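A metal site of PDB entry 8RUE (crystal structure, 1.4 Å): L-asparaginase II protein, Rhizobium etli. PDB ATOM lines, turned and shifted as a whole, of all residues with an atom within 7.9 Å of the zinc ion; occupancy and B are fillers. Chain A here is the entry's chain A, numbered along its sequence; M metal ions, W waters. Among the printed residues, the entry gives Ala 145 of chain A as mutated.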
ATOM      1  N   ARG A  53      27.269  21.677  23.252  1.00  0.00           N
ATOM      2  CA  ARG A  53      27.029  22.942  23.968  1.00  0.00           C
ATOM      3  C   ARG A  53      27.876  24.035  23.332  1.00  0.00           C
ATOM      4  O   ARG A  53      27.925  24.132  22.087  1.00  0.00           O
ATOM      5  CB  ARG A  53      27.244  22.721  25.470  1.00  0.00           C
ATOM      6  CG  ARG A  53      26.426  21.546  26.041  1.00  0.00           C
ATOM      7  CD  ARG A  53      24.909  21.802  26.075  1.00  0.00           C
ATOM      8  NE  ARG A  53      24.578  22.905  26.965  1.00  0.00           N
ATOM      9  CZ  ARG A  53      24.585  22.783  28.278  1.00  0.00           C
ATOM     10  NH1 ARG A  53      24.872  21.625  28.868  1.00  0.00           N
ATOM     11  NH2 ARG A  53      24.329  23.856  29.025  1.00  0.00           N
ATOM     12  N   SER A  54      28.575  24.868  24.121  1.00  0.00           N
ATOM     13  CA  SER A  54      29.369  25.958  23.578  1.00  0.00           C
ATOM     14  C   SER A  54      30.518  25.497  22.725  1.00  0.00           C
ATOM     15  O   SER A  54      31.039  26.295  21.938  1.00  0.00           O
ATOM     16  CB  SER A  54      29.913  26.840  24.686  1.00  0.00           C
ATOM     17  OG  SER A  54      28.865  27.589  25.299  1.00  0.00           O
ATOM     18  N   LYS A  57      30.154  26.404  19.086  1.00  0.00           N
ATOM     19  CA  LYS A  57      30.063  27.800  18.649  1.00  0.00           C
ATOM     20  C   LYS A  57      30.852  28.127  17.381  1.00  0.00           C
ATOM     21  O   LYS A  57      30.345  28.925  16.580  1.00  0.00           O
ATOM     22  CB  LYS A  57      30.416  28.745  19.823  1.00  0.00           C
ATOM     23  CG  LYS A  57      29.288  28.894  20.830  1.00  0.00           C
ATOM     24  CD  LYS A  57      29.706  29.648  22.095  1.00  0.00           C
ATOM     25  CE  LYS A  57      28.494  29.899  22.985  1.00  0.00           C
ATOM     26  NZ  LYS A  57      28.850  30.307  24.386  1.00  0.00           N
ATOM     27  N   GLN A  60      28.526  27.385  14.617  1.00  0.00           N
ATOM     28  CA  GLN A  60      27.470  28.381  14.520  1.00  0.00           C
ATOM     29  C   GLN A  60      28.019  29.694  13.948  1.00  0.00           C
ATOM     30  O   GLN A  60      27.336  30.366  13.146  1.00  0.00           O
ATOM     31  CB  GLN A  60      26.840  28.566  15.895  1.00  0.00           C
ATOM     32  CG  GLN A  60      26.084  27.315  16.363  1.00  0.00           C
ATOM     33  CD  GLN A  60      25.850  27.293  17.839  1.00  0.00           C
ATOM     34  OE1 GLN A  60      26.803  27.334  18.622  1.00  0.00           O
ATOM     35  NE2 GLN A  60      24.589  27.257  18.251  1.00  0.00           N
ATOM     36  N   ALA A  85      32.656  32.633  21.693  1.00  0.00           N
ATOM     37  CA  ALA A  85      33.029  32.701  23.107  1.00  0.00           C
ATOM     38  C   ALA A  85      32.015  32.069  24.056  1.00  0.00           C
ATOM     39  O   ALA A  85      30.825  32.066  23.796  1.00  0.00           O
ATOM     40  CB  ALA A  85      33.079  34.156  23.529  1.00  0.00           C
ATOM     41  N   SER A  86      32.500  31.626  25.228  1.00  0.00           N
ATOM     42  CA  SER A  86      31.727  31.510  26.501  1.00  0.00           C
ATOM     43  C   SER A  86      32.397  32.462  27.470  1.00  0.00           C
ATOM     44  O   SER A  86      33.171  32.053  28.338  1.00  0.00           O
ATOM     45  CB  SER A  86      31.723  30.120  27.082  1.00  0.00           C
ATOM     46  OG  SER A  86      31.130  29.193  26.165  1.00  0.00           O
ATOM     47  N   CYS A 113      18.638  35.895  24.360  1.00  0.00           N
ATOM     48  CA  CYS A 113      19.294  35.155  25.432  1.00  0.00           C
ATOM     49  C   CYS A 113      19.119  35.924  26.732  1.00  0.00           C
ATOM     50  O   CYS A 113      18.770  37.102  26.718  1.00  0.00           O
ATOM     51  CB  CYS A 113      20.785  34.996  25.118  1.00  0.00           C
ATOM     52  SG  CYS A 113      21.648  36.589  24.709  1.00  0.00           S
ATOM     53  N   SER A 139      25.104  37.846  28.787  1.00  0.00           N
ATOM     54  CA  SER A 139      25.184  36.403  28.573  1.00  0.00           C
ATOM     55  C   SER A 139      26.547  35.988  28.020  1.00  0.00           C
ATOM     56  O   SER A 139      27.102  36.666  27.155  1.00  0.00           O
ATOM     57  CB  SER A 139      24.087  35.974  27.594  1.00  0.00           C
ATOM     58  OG  SER A 139      24.288  34.645  27.099  1.00  0.00           O
ATOM     59  N   ASN A 140      27.043  34.830  28.488  1.00  0.00           N
ATOM     60  CA  ASN A 140      28.250  34.249  27.935  1.00  0.00           C
ATOM     61  C   ASN A 140      28.093  33.977  26.446  1.00  0.00           C
ATOM     62  O   ASN A 140      29.104  33.909  25.735  1.00  0.00           O
ATOM     63  CB  ASN A 140      28.655  32.967  28.692  1.00  0.00           C
ATOM     64  CG  ASN A 140      27.902  31.731  28.221  1.00  0.00           C
ATOM     65  OD1 ASN A 140      28.415  30.917  27.449  1.00  0.00           O
ATOM     66  ND2 ASN A 140      26.679  31.590  28.679  1.00  0.00           N
ATOM     67  N   CYS A 141      26.846  33.837  25.964  1.00  0.00           N
ATOM     68  CA  CYS A 141      26.531  33.613  24.563  1.00  0.00           C
ATOM     69  C   CYS A 141      26.129  34.887  23.833  1.00  0.00           C
ATOM     70  O   CYS A 141      25.568  34.788  22.746  1.00  0.00           O
ATOM     71  CB  CYS A 141      25.385  32.619  24.447  1.00  0.00           C
ATOM     72  SG  CYS A 141      25.793  30.949  25.099  1.00  0.00           S
ATOM     73  N   SER A 142      26.393  36.066  24.404  1.00  0.00           N
ATOM     74  CA  SER A 142      25.936  37.310  23.781  1.00  0.00           C
ATOM     75  C   SER A 142      26.525  37.537  22.388  1.00  0.00           C
ATOM     76  O   SER A 142      25.841  38.074  21.515  1.00  0.00           O
ATOM     77  CB  SER A 142      26.238  38.495  24.714  1.00  0.00           C
ATOM     78  OG  SER A 142      27.653  38.689  24.820  1.00  0.00           O
ATOM     79  N   LYS A 144      27.409  35.200  20.104  1.00  0.00           N
ATOM     80  CA  LYS A 144      26.667  34.325  19.201  1.00  0.00           C
ATOM     81  C   LYS A 144      25.288  34.891  18.941  1.00  0.00           C
ATOM     82  O   LYS A 144      24.819  34.896  17.795  1.00  0.00           O
ATOM     83  CB  LYS A 144      26.543  32.958  19.867  1.00  0.00           C
ATOM     84  CG  LYS A 144      25.647  32.009  19.104  1.00  0.00           C
ATOM     85  CD  LYS A 144      25.605  30.601  19.728  1.00  0.00           C
ATOM     86  CE  LYS A 144      25.221  30.694  21.217  1.00  0.00           C
ATOM     87  NZ  LYS A 144      24.927  29.374  21.905  1.00  0.00           N
ATOM     88  N   ALA A 145      24.633  35.422  19.986  1.00  0.00           N
ATOM     89  CA  ALA A 145      23.311  36.023  19.836  1.00  0.00           C
ATOM     90  C   ALA A 145      23.340  37.184  18.854  1.00  0.00           C
ATOM     91  O   ALA A 145      22.486  37.279  17.979  1.00  0.00           O
ATOM     92  CB  ALA A 145      22.781  36.476  21.203  1.00  0.00           C
ATOM     93  N   ASP A 193      19.486  25.125  24.534  1.00  0.00           N
ATOM     94  CA  ASP A 193      20.632  25.510  25.369  1.00  0.00           C
ATOM     95  C   ASP A 193      20.212  26.450  26.505  1.00  0.00           C
ATOM     96  O   ASP A 193      19.085  26.947  26.557  1.00  0.00           O
ATOM     97  CB  ASP A 193      21.700  26.189  24.489  1.00  0.00           C
ATOM     98  CG  ASP A 193      23.090  25.687  24.717  1.00  0.00           C
ATOM     99  OD1 ASP A 193      23.361  25.233  25.845  1.00  0.00           O
ATOM    100  OD2 ASP A 193      23.925  25.783  23.759  1.00  0.00           O
ATOM    101  N   GLY A 194      21.178  26.748  27.381  1.00  0.00           N
ATOM    102  CA  GLY A 194      20.950  27.726  28.438  1.00  0.00           C
ATOM    103  C   GLY A 194      20.575  29.091  27.927  1.00  0.00           C
ATOM    104  O   GLY A 194      19.833  29.816  28.595  1.00  0.00           O
ATOM    105  N   CYS A 195      21.089  29.481  26.761  1.00  0.00           N
ATOM    106  CA  CYS A 195      20.785  30.759  26.150  1.00  0.00           C
ATOM    107  C   CYS A 195      19.491  30.750  25.341  1.00  0.00           C
ATOM    108  O   CYS A 195      19.118  31.792  24.752  1.00  0.00           O
ATOM    109  CB  CYS A 195      21.964  31.189  25.266  1.00  0.00           C
ATOM    110  SG  CYS A 195      22.237  29.979  23.895  1.00  0.00           S
ATOM    111  N   ASN A 196      18.810  29.606  25.271  1.00  0.00           N
ATOM    112  CA  ASN A 196      17.490  29.423  24.633  1.00  0.00           C
ATOM    113  C   ASN A 196      17.587  29.219  23.121  1.00  0.00           C
ATOM    114  O   ASN A 196      16.535  29.267  22.456  1.00  0.00           O
ATOM    115  CB  ASN A 196      16.444  30.497  24.990  1.00  0.00           C
ATOM    116  CG  ASN A 196      15.020  29.943  25.048  1.00  0.00           C
ATOM    117  OD1 ASN A 196      14.799  28.771  25.397  1.00  0.00           O
ATOM    118  ND2 ASN A 196      14.057  30.770  24.653  1.00  0.00           N
ATOM    119  N   LEU A 197      18.787  28.958  22.556  1.00  0.00           N
ATOM    120  CA  LEU A 197      18.985  28.572  21.157  1.00  0.00           C
ATOM    121  C   LEU A 197      18.978  27.058  21.002  1.00  0.00           C
ATOM    122  O   LEU A 197      19.290  26.327  21.952  1.00  0.00           O
ATOM    123  CB  LEU A 197      20.346  29.073  20.679  1.00  0.00           C
ATOM    124  CG  LEU A 197      20.440  30.539  20.254  1.00  0.00           C
ATOM    125  CD1 LEU A 197      21.874  30.938  20.124  1.00  0.00           C
ATOM    126  CD2 LEU A 197      19.749  30.701  18.931  1.00  0.00           C
ATOM    127  N   PRO A 198      18.645  26.551  19.820  1.00  0.00           N
ATOM    128  CA  PRO A 198      18.885  25.120  19.558  1.00  0.00           C
ATOM    129  C   PRO A 198      20.360  24.784  19.763  1.00  0.00           C
ATOM    130  O   PRO A 198      21.253  25.597  19.459  1.00  0.00           O
ATOM    131  CB  PRO A 198      18.509  24.955  18.085  1.00  0.00           C
ATOM    132  CG  PRO A 198      17.603  26.145  17.797  1.00  0.00           C
ATOM    133  CD  PRO A 198      18.181  27.253  18.608  1.00  0.00           C
ATOM    134  N   THR A 199      20.615  23.579  20.289  1.00  0.00           N
ATOM    135  CA  THR A 199      21.999  23.134  20.535  1.00  0.00           C
ATOM    136  C   THR A 199      22.138  21.662  20.135  1.00  0.00           C
ATOM    137  O   THR A 199      21.238  20.839  20.399  1.00  0.00           O
ATOM    138  CB  THR A 199      22.366  23.379  22.019  1.00  0.00           C
ATOM    139  OG1 THR A 199      23.773  23.228  22.212  1.00  0.00           O
ATOM    140  CG2 THR A 199      21.567  22.490  23.026  1.00  0.00           C
HETATM  141 ZN    ZN M   1      24.465  29.538  23.904  1.00  0.00          ZN
HETATM  142  O   HOH W   1      25.491  27.825  24.518  1.00  0.00           O
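The guanidinium group (NE) of Arg 53 is in salt-bridge range of the side-chain carboxylate (OD1) of Asp 193, at 2.9 Å.
The side-chain amide oxygen (OD1) of Asn 140 sits close to the side-chain sulfur (SG) of Cys 141, 3.5 Å away.
SG of Cys 141 lies close to NZ of Lys 57.
OG of Ser 139 is in hydrogen-bond range of N of Cys 141, at 2.9 Å.
The side-chain carboxylate of Asp 193 sits at hydrogen-bond distance from the side-chain hydroxyl of Thr 199, 3.0 Å away.
Residues that only touch the zinc ion: Asp 193.
Four residues have an atom within 4 Å of the zinc ion: Cys 141, Lys 144, Asp 193 and Cys 195.
The zinc ion is bound by NZ of Lys 144 (2.1 Å), water W1 (2.1 Å), SG of Cys 195 (2.3 Å) and SG of Cys 141 (2.3 Å).
Water W1 lies within hydrogen-bond range of the side-chain carboxylate of Asp 193 (2.7 Å) and the side-chain hydroxyl of Ser 54 (3.5 Å).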
